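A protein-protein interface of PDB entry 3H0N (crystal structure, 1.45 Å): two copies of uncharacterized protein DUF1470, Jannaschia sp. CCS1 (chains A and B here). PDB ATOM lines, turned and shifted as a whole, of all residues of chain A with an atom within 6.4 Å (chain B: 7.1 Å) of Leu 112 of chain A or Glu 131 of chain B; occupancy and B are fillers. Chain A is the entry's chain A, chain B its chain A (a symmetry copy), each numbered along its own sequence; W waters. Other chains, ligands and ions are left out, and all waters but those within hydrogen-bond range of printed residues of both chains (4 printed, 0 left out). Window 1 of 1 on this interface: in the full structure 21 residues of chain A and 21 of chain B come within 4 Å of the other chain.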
ATOM      1  N   TYR A   7      -1.329  36.701 -33.052  1.00  0.00           N
ATOM      2  CA  TYR A   7      -2.390  35.743 -33.273  1.00  0.00           C
ATOM      3  C   TYR A   7      -3.373  35.778 -32.116  1.00  0.00           C
ATOM      4  O   TYR A   7      -4.575  35.685 -32.296  1.00  0.00           O
ATOM      5  CB  TYR A   7      -1.827  34.300 -33.480  1.00  0.00           C
ATOM      6  CG  TYR A   7      -2.920  33.266 -33.583  1.00  0.00           C
ATOM      7  CD1 TYR A   7      -3.562  32.995 -34.798  1.00  0.00           C
ATOM      8  CD2 TYR A   7      -3.366  32.627 -32.455  1.00  0.00           C
ATOM      9  CE1 TYR A   7      -4.613  32.063 -34.849  1.00  0.00           C
ATOM     10  CE2 TYR A   7      -4.420  31.742 -32.490  1.00  0.00           C
ATOM     11  CZ  TYR A   7      -5.043  31.460 -33.686  1.00  0.00           C
ATOM     12  OH  TYR A   7      -6.115  30.604 -33.750  1.00  0.00           O
ATOM     13  N   PRO A 100     -13.464  25.605 -29.043  1.00  0.00           N
ATOM     14  CA  PRO A 100     -12.083  25.724 -29.520  1.00  0.00           C
ATOM     15  C   PRO A 100     -11.512  24.451 -30.115  1.00  0.00           C
ATOM     16  O   PRO A 100     -11.953  23.344 -29.773  1.00  0.00           O
ATOM     17  CB  PRO A 100     -11.311  26.135 -28.292  1.00  0.00           C
ATOM     18  CG  PRO A 100     -12.278  26.359 -27.225  1.00  0.00           C
ATOM     19  CD  PRO A 100     -13.565  25.738 -27.594  1.00  0.00           C
ATOM     20  N   GLU A 101     -10.503  24.617 -30.953  1.00  0.00           N
ATOM     21  CA  GLU A 101      -9.855  23.497 -31.633  1.00  0.00           C
ATOM     22  C   GLU A 101      -8.399  23.867 -31.921  1.00  0.00           C
ATOM     23  O   GLU A 101      -8.113  24.914 -32.518  1.00  0.00           O
ATOM     24  CB  GLU A 101     -10.617  23.148 -32.937  1.00  0.00           C
ATOM     25  CG  GLU A 101     -10.036  21.932 -33.663  1.00  0.00           C
ATOM     26  CD  GLU A 101     -10.822  21.457 -34.897  1.00  0.00           C
ATOM     27  OE1 GLU A 101     -11.994  21.845 -35.057  1.00  0.00           O
ATOM     28  OE2 GLU A 101     -10.254  20.625 -35.679  1.00  0.00           O
ATOM     29  N   LEU A 102      -7.496  22.945 -31.566  1.00  0.00           N
ATOM     30  CA  LEU A 102      -6.094  23.043 -31.929  1.00  0.00           C
ATOM     31  C   LEU A 102      -5.856  22.603 -33.348  1.00  0.00           C
ATOM     32  O   LEU A 102      -6.388  21.579 -33.777  1.00  0.00           O
ATOM     33  CB  LEU A 102      -5.245  22.187 -30.989  1.00  0.00           C
ATOM     34  CG  LEU A 102      -5.125  22.637 -29.540  1.00  0.00           C
ATOM     35  CD1 LEU A 102      -4.731  21.454 -28.655  1.00  0.00           C
ATOM     36  CD2 LEU A 102      -4.126  23.795 -29.428  1.00  0.00           C
ATOM     37  N   ALA A 103      -4.993  23.331 -34.050  1.00  0.00           N
ATOM     38  CA  ALA A 103      -4.553  22.903 -35.387  1.00  0.00           C
ATOM     39  C   ALA A 103      -3.185  23.446 -35.680  1.00  0.00           C
ATOM     40  O   ALA A 103      -2.765  24.432 -35.072  1.00  0.00           O
ATOM     41  CB  ALA A 103      -5.566  23.382 -36.457  1.00  0.00           C
ATOM     42  N   TRP A 110       1.539  25.300 -33.834  1.00  0.00           N
ATOM     43  CA  TRP A 110       0.255  24.945 -33.261  1.00  0.00           C
ATOM     44  C   TRP A 110      -0.457  26.196 -32.752  1.00  0.00           C
ATOM     45  O   TRP A 110       0.153  27.071 -32.119  1.00  0.00           O
ATOM     46  CB  TRP A 110       0.440  23.992 -32.079  1.00  0.00           C
ATOM     47  CG  TRP A 110       0.819  22.662 -32.496  1.00  0.00           C
ATOM     48  CD1 TRP A 110       2.101  22.148 -32.598  1.00  0.00           C
ATOM     49  CD2 TRP A 110      -0.058  21.623 -32.941  1.00  0.00           C
ATOM     50  NE1 TRP A 110       2.050  20.867 -33.045  1.00  0.00           N
ATOM     51  CE2 TRP A 110       0.747  20.504 -33.268  1.00  0.00           C
ATOM     52  CE3 TRP A 110      -1.446  21.520 -33.098  1.00  0.00           C
ATOM     53  CZ2 TRP A 110       0.202  19.322 -33.743  1.00  0.00           C
ATOM     54  CZ3 TRP A 110      -1.984  20.336 -33.558  1.00  0.00           C
ATOM     55  CH2 TRP A 110      -1.161  19.254 -33.880  1.00  0.00           C
ATOM     56  N   ARG A 111      -1.748  26.286 -33.042  1.00  0.00           N
ATOM     57  CA  ARG A 111      -2.606  27.407 -32.657  1.00  0.00           C
ATOM     58  C   ARG A 111      -3.873  26.894 -32.038  1.00  0.00           C
ATOM     59  O   ARG A 111      -4.414  25.880 -32.490  1.00  0.00           O
ATOM     60  CB  ARG A 111      -2.991  28.267 -33.846  1.00  0.00           C
ATOM     61  CG  ARG A 111      -1.876  28.736 -34.749  1.00  0.00           C
ATOM     62  CD  ARG A 111      -1.195  29.861 -34.121  1.00  0.00           C
ATOM     63  NE  ARG A 111      -0.193  30.440 -35.022  1.00  0.00           N
ATOM     64  CZ  ARG A 111       0.691  31.341 -34.611  1.00  0.00           C
ATOM     65  NH1 ARG A 111       0.685  31.763 -33.357  1.00  0.00           N
ATOM     66  NH2 ARG A 111       1.601  31.803 -35.470  1.00  0.00           N
ATOM     67  N   LEU A 112      -4.386  27.618 -31.049  1.00  0.00           N
ATOM     68  CA  LEU A 112      -5.738  27.372 -30.527  1.00  0.00           C
ATOM     69  C   LEU A 112      -6.699  28.274 -31.269  1.00  0.00           C
ATOM     70  O   LEU A 112      -6.609  29.511 -31.162  1.00  0.00           O
ATOM     71  CB  LEU A 112      -5.835  27.647 -29.030  1.00  0.00           C
ATOM     72  CG  LEU A 112      -7.179  27.298 -28.374  1.00  0.00           C
ATOM     73  CD1 LEU A 112      -7.610  25.812 -28.575  1.00  0.00           C
ATOM     74  CD2 LEU A 112      -7.190  27.667 -26.905  1.00  0.00           C
ATOM     75  N   HIS A 113      -7.597  27.692 -32.055  1.00  0.00           N
ATOM     76  CA  HIS A 113      -8.638  28.424 -32.773  1.00  0.00           C
ATOM     77  C   HIS A 113      -9.855  28.485 -31.907  1.00  0.00           C
ATOM     78  O   HIS A 113     -10.224  27.514 -31.282  1.00  0.00           O
ATOM     79  CB  HIS A 113      -8.955  27.703 -34.072  1.00  0.00           C
ATOM     80  CG  HIS A 113      -7.796  27.693 -35.014  1.00  0.00           C
ATOM     81  ND1 HIS A 113      -7.598  28.688 -35.957  1.00  0.00           N
ATOM     82  CD2 HIS A 113      -6.737  26.853 -35.121  1.00  0.00           C
ATOM     83  CE1 HIS A 113      -6.469  28.439 -36.609  1.00  0.00           C
ATOM     84  NE2 HIS A 113      -5.924  27.334 -36.121  1.00  0.00           N
ATOM     85  N   HIS A 114     -10.518  29.637 -31.859  1.00  0.00           N
ATOM     86  CA  HIS A 114     -11.701  29.845 -31.019  1.00  0.00           C
ATOM     87  C   HIS A 114     -12.982  29.601 -31.787  1.00  0.00           C
ATOM     88  O   HIS A 114     -13.948  30.360 -31.707  1.00  0.00           O
ATOM     89  CB  HIS A 114     -11.602  31.223 -30.377  1.00  0.00           C
ATOM     90  CG  HIS A 114     -10.521  31.260 -29.379  1.00  0.00           C
ATOM     91  ND1 HIS A 114      -9.239  31.641 -29.686  1.00  0.00           N
ATOM     92  CD2 HIS A 114     -10.498  30.824 -28.107  1.00  0.00           C
ATOM     93  CE1 HIS A 114      -8.478  31.485 -28.611  1.00  0.00           C
ATOM     94  NE2 HIS A 114      -9.221  30.988 -27.633  1.00  0.00           N
ATOM     95  N   HIS A 115     -12.957  28.468 -32.480  1.00  0.00           N
ATOM     96  CA  HIS A 115     -14.058  27.973 -33.305  1.00  0.00           C
ATOM     97  C   HIS A 115     -13.600  26.607 -33.817  1.00  0.00           C
ATOM     98  O   HIS A 115     -12.402  26.353 -33.925  1.00  0.00           O
ATOM     99  CB  HIS A 115     -14.311  28.903 -34.508  1.00  0.00           C
ATOM    100  CG  HIS A 115     -13.106  29.033 -35.376  1.00  0.00           C
ATOM    101  ND1 HIS A 115     -12.897  28.224 -36.469  1.00  0.00           N
ATOM    102  CD2 HIS A 115     -12.017  29.833 -35.288  1.00  0.00           C
ATOM    103  CE1 HIS A 115     -11.713  28.491 -36.984  1.00  0.00           C
ATOM    104  NE2 HIS A 115     -11.172  29.487 -36.296  1.00  0.00           N
ATOM    105  N   GLU B   8      -7.121  32.858 -14.479  1.00  0.00           N
ATOM    106  CA  GLU B   8      -6.832  32.616 -15.881  1.00  0.00           C
ATOM    107  C   GLU B   8      -6.096  31.310 -16.150  1.00  0.00           C
ATOM    108  O   GLU B   8      -6.191  30.770 -17.255  1.00  0.00           O
ATOM    109  CB  GLU B   8      -6.003  33.794 -16.459  1.00  0.00           C
ATOM    110  CG  GLU B   8      -6.815  35.054 -16.628  1.00  0.00           C
ATOM    111  CD  GLU B   8      -7.065  35.843 -15.332  1.00  0.00           C
ATOM    112  OE1 GLU B   8      -6.414  35.613 -14.274  1.00  0.00           O
ATOM    113  OE2 GLU B   8      -7.916  36.768 -15.394  1.00  0.00           O
ATOM    114  N   GLY B  11      -7.516  26.060 -15.480  1.00  0.00           N
ATOM    115  CA  GLY B  11      -7.521  24.781 -16.159  1.00  0.00           C
ATOM    116  C   GLY B  11      -6.172  24.111 -16.106  1.00  0.00           C
ATOM    117  O   GLY B  11      -6.077  22.910 -15.871  1.00  0.00           O
ATOM    118  N   LEU B  12      -5.135  24.895 -16.324  1.00  0.00           N
ATOM    119  CA  LEU B  12      -3.770  24.355 -16.226  1.00  0.00           C
ATOM    120  C   LEU B  12      -3.472  23.852 -14.832  1.00  0.00           C
ATOM    121  O   LEU B  12      -2.958  22.715 -14.626  1.00  0.00           O
ATOM    122  CB  LEU B  12      -2.730  25.424 -16.648  1.00  0.00           C
ATOM    123  CG  LEU B  12      -1.247  25.070 -16.508  1.00  0.00           C
ATOM    124  CD1 LEU B  12      -0.900  23.870 -17.413  1.00  0.00           C
ATOM    125  CD2 LEU B  12      -0.389  26.289 -16.847  1.00  0.00           C
ATOM    126  N   SER B  15      -5.539  20.797 -13.847  1.00  0.00           N
ATOM    127  CA  SER B  15      -5.071  19.626 -14.616  1.00  0.00           C
ATOM    128  C   SER B  15      -3.841  18.999 -13.942  1.00  0.00           C
ATOM    129  O   SER B  15      -3.793  17.792 -13.717  1.00  0.00           O
ATOM    130  CB  SER B  15      -4.651  20.024 -16.037  1.00  0.00           C
ATOM    131  OG  SER B  15      -5.760  20.366 -16.848  1.00  0.00           O
ATOM    132  N   LEU B  89      -7.126  16.377 -26.789  1.00  0.00           N
ATOM    133  CA  LEU B  89      -7.758  17.578 -26.241  1.00  0.00           C
ATOM    134  C   LEU B  89      -8.905  18.077 -27.132  1.00  0.00           C
ATOM    135  O   LEU B  89      -9.960  18.473 -26.638  1.00  0.00           O
ATOM    136  CB  LEU B  89      -6.710  18.673 -26.044  1.00  0.00           C
ATOM    137  CG  LEU B  89      -5.633  18.384 -24.986  1.00  0.00           C
ATOM    138  CD1 LEU B  89      -4.483  19.369 -25.087  1.00  0.00           C
ATOM    139  CD2 LEU B  89      -6.216  18.386 -23.558  1.00  0.00           C
ATOM    140  N   ASN B  90      -8.728  17.994 -28.447  1.00  0.00           N
ATOM    141  CA  ASN B  90      -9.787  18.406 -29.388  1.00  0.00           C
ATOM    142  C   ASN B  90     -11.029  17.574 -29.215  1.00  0.00           C
ATOM    143  O   ASN B  90     -12.137  18.086 -29.290  1.00  0.00           O
ATOM    144  CB  ASN B  90      -9.307  18.349 -30.833  1.00  0.00           C
ATOM    145  CG  ASN B  90      -8.394  19.475 -31.194  1.00  0.00           C
ATOM    146  OD1 ASN B  90      -8.334  20.488 -30.487  1.00  0.00           O
ATOM    147  ND2 ASN B  90      -7.747  19.364 -32.358  1.00  0.00           N
ATOM    148  N   LEU B  92     -11.998  16.084 -26.427  1.00  0.00           N
ATOM    149  CA  LEU B  92     -12.642  16.507 -25.169  1.00  0.00           C
ATOM    150  C   LEU B  92     -13.435  17.807 -25.321  1.00  0.00           C
ATOM    151  O   LEU B  92     -14.527  17.935 -24.756  1.00  0.00           O
ATOM    152  CB  LEU B  92     -11.629  16.625 -24.035  1.00  0.00           C
ATOM    153  CG  LEU B  92     -10.931  15.331 -23.656  1.00  0.00           C
ATOM    154  CD1 LEU B  92      -9.866  15.695 -22.667  1.00  0.00           C
ATOM    155  CD2 LEU B  92     -11.960  14.329 -23.106  1.00  0.00           C
ATOM    156  N   LEU B  93     -12.890  18.736 -26.092  1.00  0.00           N
ATOM    157  CA  LEU B  93     -13.542  20.024 -26.331  1.00  0.00           C
ATOM    158  C   LEU B  93     -14.814  19.849 -27.173  1.00  0.00           C
ATOM    159  O   LEU B  93     -15.801  20.558 -26.978  1.00  0.00           O
ATOM    160  CB  LEU B  93     -12.565  21.018 -26.992  1.00  0.00           C
ATOM    161  CG  LEU B  93     -11.448  21.436 -26.019  1.00  0.00           C
ATOM    162  CD1 LEU B  93     -10.255  22.007 -26.801  1.00  0.00           C
ATOM    163  CD2 LEU B  93     -12.003  22.383 -24.942  1.00  0.00           C
ATOM    164  N   ALA B  98     -17.975  23.433 -24.148  1.00  0.00           N
ATOM    165  CA  ALA B  98     -16.835  24.320 -24.094  1.00  0.00           C
ATOM    166  C   ALA B  98     -17.120  25.737 -24.623  1.00  0.00           C
ATOM    167  O   ALA B  98     -16.193  26.537 -24.724  1.00  0.00           O
ATOM    168  CB  ALA B  98     -15.655  23.696 -24.805  1.00  0.00           C
ATOM    169  N   HIS B 114     -14.874  29.076 -19.345  1.00  0.00           N
ATOM    170  CA  HIS B 114     -14.628  28.261 -20.538  1.00  0.00           C
ATOM    171  C   HIS B 114     -15.563  27.072 -20.605  1.00  0.00           C
ATOM    172  O   HIS B 114     -15.167  25.944 -20.900  1.00  0.00           O
ATOM    173  CB  HIS B 114     -13.147  27.905 -20.584  1.00  0.00           C
ATOM    174  CG  HIS B 114     -12.331  29.097 -20.866  1.00  0.00           C
ATOM    175  ND1 HIS B 114     -11.803  29.887 -19.877  1.00  0.00           N
ATOM    176  CD2 HIS B 114     -12.071  29.715 -22.032  1.00  0.00           C
ATOM    177  CE1 HIS B 114     -11.198  30.926 -20.437  1.00  0.00           C
ATOM    178  NE2 HIS B 114     -11.347  30.846 -21.751  1.00  0.00           N
ATOM    179  N   TRP B 125     -15.539  20.530 -15.779  1.00  0.00           N
ATOM    180  CA  TRP B 125     -14.107  20.473 -15.429  1.00  0.00           C
ATOM    181  C   TRP B 125     -13.283  19.847 -16.541  1.00  0.00           C
ATOM    182  O   TRP B 125     -12.157  20.278 -16.753  1.00  0.00           O
ATOM    183  CB  TRP B 125     -13.905  19.833 -14.050  1.00  0.00           C
ATOM    184  CG  TRP B 125     -14.239  20.824 -12.978  1.00  0.00           C
ATOM    185  CD1 TRP B 125     -15.363  20.887 -12.248  1.00  0.00           C
ATOM    186  CD2 TRP B 125     -13.467  21.984 -12.662  1.00  0.00           C
ATOM    187  NE1 TRP B 125     -15.333  22.015 -11.431  1.00  0.00           N
ATOM    188  CE2 TRP B 125     -14.178  22.706 -11.683  1.00  0.00           C
ATOM    189  CE3 TRP B 125     -12.237  22.469 -13.103  1.00  0.00           C
ATOM    190  CZ2 TRP B 125     -13.698  23.913 -11.146  1.00  0.00           C
ATOM    191  CZ3 TRP B 125     -11.775  23.663 -12.568  1.00  0.00           C
ATOM    192  CH2 TRP B 125     -12.492  24.361 -11.617  1.00  0.00           C
ATOM    193  N   THR B 126     -13.855  18.928 -17.307  1.00  0.00           N
ATOM    194  CA  THR B 126     -13.197  18.399 -18.484  1.00  0.00           C
ATOM    195  C   THR B 126     -12.936  19.502 -19.486  1.00  0.00           C
ATOM    196  O   THR B 126     -11.816  19.625 -20.005  1.00  0.00           O
ATOM    197  CB  THR B 126     -14.003  17.260 -19.117  1.00  0.00           C
ATOM    198  OG1 THR B 126     -14.162  16.216 -18.152  1.00  0.00           O
ATOM    199  CG2 THR B 126     -13.260  16.704 -20.329  1.00  0.00           C
ATOM    200  N   ALA B 127     -13.931  20.337 -19.774  1.00  0.00           N
ATOM    201  CA  ALA B 127     -13.749  21.444 -20.702  1.00  0.00           C
ATOM    202  C   ALA B 127     -12.757  22.464 -20.211  1.00  0.00           C
ATOM    203  O   ALA B 127     -11.944  22.982 -21.005  1.00  0.00           O
ATOM    204  CB  ALA B 127     -15.130  22.123 -20.969  1.00  0.00           C
ATOM    205  N   ILE B 128     -12.821  22.801 -18.927  1.00  0.00           N
ATOM    206  CA  ILE B 128     -11.916  23.792 -18.355  1.00  0.00           C
ATOM    207  C   ILE B 128     -10.479  23.306 -18.461  1.00  0.00           C
ATOM    208  O   ILE B 128      -9.562  24.047 -18.871  1.00  0.00           O
ATOM    209  CB  ILE B 128     -12.270  24.075 -16.897  1.00  0.00           C
ATOM    210  CG1 ILE B 128     -13.621  24.838 -16.815  1.00  0.00           C
ATOM    211  CG2 ILE B 128     -11.212  24.953 -16.205  1.00  0.00           C
ATOM    212  CD1 ILE B 128     -14.193  24.931 -15.398  1.00  0.00           C
ATOM    213  N   CYS B 129     -10.277  22.071 -18.062  1.00  0.00           N
ATOM    214  CA  CYS B 129      -8.925  21.502 -18.074  1.00  0.00           C
ATOM    215  C   CYS B 129      -8.394  21.367 -19.484  1.00  0.00           C
ATOM    216  O   CYS B 129      -7.242  21.724 -19.756  1.00  0.00           O
ATOM    217  CB  CYS B 129      -8.895  20.156 -17.360  1.00  0.00           C
ATOM    218  SG  CYS B 129      -9.093  20.289 -15.556  1.00  0.00           S
ATOM    219  N   ALA B 130      -9.238  20.887 -20.392  1.00  0.00           N
ATOM    220  CA  ALA B 130      -8.805  20.711 -21.777  1.00  0.00           C
ATOM    221  C   ALA B 130      -8.419  22.024 -22.430  1.00  0.00           C
ATOM    222  O   ALA B 130      -7.419  22.131 -23.107  1.00  0.00           O
ATOM    223  CB  ALA B 130      -9.877  19.971 -22.660  1.00  0.00           C
ATOM    224  N   GLU B 131      -9.266  23.045 -22.238  1.00  0.00           N
ATOM    225  CA  GLU B 131      -8.944  24.374 -22.802  1.00  0.00           C
ATOM    226  C   GLU B 131      -7.642  24.916 -22.196  1.00  0.00           C
ATOM    227  O   GLU B 131      -6.822  25.531 -22.865  1.00  0.00           O
ATOM    228  CB  GLU B 131     -10.087  25.387 -22.659  1.00  0.00           C
ATOM    229  CG  GLU B 131      -9.815  26.743 -23.349  1.00  0.00           C
ATOM    230  CD  GLU B 131      -8.922  27.713 -22.570  1.00  0.00           C
ATOM    231  OE1 GLU B 131      -8.819  27.603 -21.321  1.00  0.00           O
ATOM    232  OE2 GLU B 131      -8.326  28.615 -23.234  1.00  0.00           O
ATOM    233  N   GLY B 132      -7.449  24.685 -20.901  1.00  0.00           N
ATOM    234  CA  GLY B 132      -6.250  25.224 -20.233  1.00  0.00           C
ATOM    235  C   GLY B 132      -4.975  24.626 -20.803  1.00  0.00           C
ATOM    236  O   GLY B 132      -3.985  25.327 -21.093  1.00  0.00           O
ATOM    237  N   LEU B 133      -4.994  23.316 -21.003  1.00  0.00           N
ATOM    238  CA  LEU B 133      -3.840  22.665 -21.639  1.00  0.00           C
ATOM    239  C   LEU B 133      -3.686  23.085 -23.084  1.00  0.00           C
ATOM    240  O   LEU B 133      -2.580  23.376 -23.554  1.00  0.00           O
ATOM    241  CB  LEU B 133      -3.903  21.150 -21.528  1.00  0.00           C
ATOM    242  CG  LEU B 133      -3.835  20.623 -20.121  1.00  0.00           C
ATOM    243  CD1 LEU B 133      -3.982  19.099 -20.163  1.00  0.00           C
ATOM    244  CD2 LEU B 133      -2.594  21.039 -19.366  1.00  0.00           C
ATOM    245  N   ALA B 134      -4.796  23.123 -23.817  1.00  0.00           N
ATOM    246  CA  ALA B 134      -4.777  23.549 -25.225  1.00  0.00           C
ATOM    247  C   ALA B 134      -4.184  24.951 -25.385  1.00  0.00           C
ATOM    248  O   ALA B 134      -3.445  25.229 -26.336  1.00  0.00           O
ATOM    249  CB  ALA B 134      -6.176  23.455 -25.876  1.00  0.00           C
ATOM    250  N   ARG B 135      -4.562  25.840 -24.484  1.00  0.00           N
ATOM    251  CA  ARG B 135      -4.088  27.217 -24.553  1.00  0.00           C
ATOM    252  C   ARG B 135      -2.588  27.306 -24.439  1.00  0.00           C
ATOM    253  O   ARG B 135      -1.916  28.082 -25.105  1.00  0.00           O
ATOM    254  CB  ARG B 135      -4.796  28.065 -23.510  1.00  0.00           C
ATOM    255  CG  ARG B 135      -4.584  29.538 -23.745  1.00  0.00           C
ATOM    256  CD  ARG B 135      -4.974  30.395 -22.591  1.00  0.00           C
ATOM    257  NE  ARG B 135      -6.155  29.966 -21.884  1.00  0.00           N
ATOM    258  CZ  ARG B 135      -6.352  30.219 -20.594  1.00  0.00           C
ATOM    259  NH1 ARG B 135      -5.518  30.965 -19.920  1.00  0.00           N
ATOM    260  NH2 ARG B 135      -7.415  29.732 -19.990  1.00  0.00           N
ATOM    261  N   GLU B 136      -2.016  26.492 -23.548  1.00  0.00           N
ATOM    262  CA  GLU B 136      -0.566  26.506 -23.398  1.00  0.00           C
ATOM    263  C   GLU B 136       0.176  25.945 -24.618  1.00  0.00           C
ATOM    264  O   GLU B 136       1.275  26.391 -24.927  1.00  0.00           O
ATOM    265  CB  GLU B 136      -0.131  25.752 -22.137  1.00  0.00           C
ATOM    266  CG  GLU B 136      -0.643  26.340 -20.817  1.00  0.00           C
ATOM    267  CD  GLU B 136      -0.377  27.802 -20.618  1.00  0.00           C
ATOM    268  OE1 GLU B 136       0.606  28.323 -21.199  1.00  0.00           O
ATOM    269  OE2 GLU B 136      -1.187  28.439 -19.886  1.00  0.00           O
ATOM    270  N   ILE B 137      -0.439  24.992 -25.327  1.00  0.00           N
ATOM    271  CA  ILE B 137       0.106  24.519 -26.589  1.00  0.00           C
ATOM    272  C   ILE B 137       0.077  25.690 -27.598  1.00  0.00           C
ATOM    273  O   ILE B 137       1.057  25.984 -28.263  1.00  0.00           O
ATOM    274  CB  ILE B 137      -0.688  23.314 -27.126  1.00  0.00           C
ATOM    275  CG1 ILE B 137      -0.593  22.098 -26.171  1.00  0.00           C
ATOM    276  CG2 ILE B 137      -0.275  22.958 -28.561  1.00  0.00           C
ATOM    277  CD1 ILE B 137      -1.583  20.968 -26.516  1.00  0.00           C
ATOM    278  N   GLY B 138      -1.052  26.398 -27.676  1.00  0.00           N
ATOM    279  CA  GLY B 138      -1.139  27.551 -28.562  1.00  0.00           C
ATOM    280  C   GLY B 138      -0.165  28.632 -28.233  1.00  0.00           C
ATOM    281  O   GLY B 138       0.340  29.341 -29.134  1.00  0.00           O
ATOM    282  N   HIS B 139       0.142  28.784 -26.952  1.00  0.00           N
ATOM    283  CA  HIS B 139       1.095  29.807 -26.502  1.00  0.00           C
ATOM    284  C   HIS B 139       2.547  29.377 -26.587  1.00  0.00           C
ATOM    285  O   HIS B 139       3.443  30.072 -26.095  1.00  0.00           O
ATOM    286  CB  HIS B 139       0.754  30.294 -25.075  1.00  0.00           C
ATOM    287  CG  HIS B 139      -0.522  31.096 -25.004  1.00  0.00           C
ATOM    288  ND1 HIS B 139      -1.083  31.520 -23.818  1.00  0.00           N
ATOM    289  CD2 HIS B 139      -1.348  31.524 -25.989  1.00  0.00           C
ATOM    290  CE1 HIS B 139      -2.182  32.214 -24.087  1.00  0.00           C
ATOM    291  NE2 HIS B 139      -2.375  32.218 -25.391  1.00  0.00           N
ATOM    292  N   GLN B 140       2.804  28.231 -27.225  1.00  0.00           N
ATOM    293  CA  GLN B 140       4.144  27.766 -27.540  1.00  0.00           C
ATOM    294  C   GLN B 140       4.925  27.404 -26.274  1.00  0.00           C
ATOM    295  O   GLN B 140       6.154  27.563 -26.211  1.00  0.00           O
ATOM    296  CB  GLN B 140       4.908  28.802 -28.374  1.00  0.00           C
ATOM    297  CG  GLN B 140       4.102  29.374 -29.574  1.00  0.00           C
ATOM    298  CD  GLN B 140       3.703  28.298 -30.525  1.00  0.00           C
ATOM    299  OE1 GLN B 140       4.549  27.627 -31.119  1.00  0.00           O
ATOM    300  NE2 GLN B 140       2.377  28.081 -30.668  1.00  0.00           N
HETATM  301  O   HOH W   1     -12.169  20.746 -30.829  1.00  0.00           O
HETATM  302  O   HOH W   2      -0.771  31.047 -30.920  1.00  0.00           O
HETATM  303  O   HOH W   3       3.818  25.156 -32.019  1.00  0.00           O
HETATM  304  O   HOH W   4      -9.460  30.005 -25.113  1.00  0.00           O
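The side-chain amide nitrogen (NE2) of Gln 140 of chain B lies within hydrogen-bond range of the backbone carbonyl oxygen (O) of Trp 110 of chain A, at 2.8 Å. OD1 of Asn 90 of chain B is in hydrogen-bond range of N of Leu 102 of chain A (2.8 Å).
O of Leu 112 of chain A lies within hydrogen-bond range of OH of Tyr 7 of chain A (2.9 Å). The side-chain carboxylate (OE1) of Glu 131 of chain B is in salt-bridge range of the guanidinium group (NH2) of Arg 135 of chain B (2.9 Å). NE2 of Gln 140 of chain B lies within hydrogen-bond range of O of Ile 137 of chain B (3.5 Å). O of Gly 138 of chain B sits at hydrogen-bond distance from NE2 of Gln 140 of chain B (2.8 Å). N of His 113 of chain A sits at hydrogen-bond distance from O of Glu 101 of chain A.
Leu 93 of chain B touches Pro 100 of chain A. Ala 98 of chain B touches Pro 100 of chain A. Asn 90 of chain B touches Glu 101 of chain A. Ala 134 of chain B touches Leu 102 of chain A. Leu 102 of chain A touches Ile 137 of chain B. Trp 110 of chain A touches Ile 137 of chain B (CB to CG2, 3.7 Å). O of Gly 138 of chain B touches O of Trp 110 of chain A (3.8 Å). OE2 of Glu 131 of chain B touches CD2 of Leu 112 of chain A, at 3.96 Å. CD1 of Leu 112 of chain A touches CB of Ala 134 of chain B, 3.9 Å away. Leu 112 of chain A touches Arg 135 of chain B (CD2 to CA, 3.9 Å).
Of the printed residues of chain B, Glu 101 of chain A touches Asn 90 (3.6 Å). Of the printed residues of chain A, Leu 93 of chain B touches Pro 100. His 114 of chain B touches none of the printed residues of chain A. Of the printed residues of chain A, Arg 135 of chain B touches Leu 112 (3.9 Å). Printed residues of chain A within 4 Å of Gly 138 of chain B: Trp 110 (3.8 Å). Printed residues of chain A within 4 Å of Gln 140 of chain B: Trp 110. The nearest residue of chain B that does not touch Leu 112 of chain A is Gly 138 of chain B (4.1 Å). The nearest residue of chain A that does not touch Glu 131 of chain B is Pro 100 of chain A (4.6 Å). The nearest printed residue of chain A that does not touch Ala 98 of chain B is His 114 of chain A (7.9 Å).
Printed residues of chain A that touch a printed residue of chain B: Pro 100, Glu 101, Leu 102, Trp 110 and Leu 112. Hydrophobic or aromatic side chains of chain A that line the printed part of chain B: Pro 100, Leu 102, Trp 110 and Leu 112. Of the 26 printed residues of chain B, 9 touch a printed residue of chain A. Hydrophobic or aromatic side chains of chain B that line the printed part of chain A: Leu 93, Ala 134 and Ile 137. Among the printed residues, no Asp or Glu carboxylate lies within 4 Å of a Lys or Arg side-chain nitrogen of the other chain.
1 position is printed for both chains. Of the 12 pairs that touch across the chains among the printed residues, none has its exchanged pair printed and touching as well.
Water W4 lies within hydrogen-bond range of OE2 of Glu 131 of chain B (2.6 Å) and NE2 of His 114 of chain A (2.7 Å). Water W2 bridges O of Gly 138 of chain B (2.7 Å) and NH1 of Arg 111 of chain A (2.9 Å). Water W3 bridges OE1 of Gln 140 of chain B (2.7 Å) and N of Trp 110 of chain A (2.9 Å). Water W1 bridges the backbone carbonyl oxygen (O) of Pro 100 of chain A (2.8 Å) and the backbone carbonyl oxygen (O) of Asn 90 of chain B (3.1 Å).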
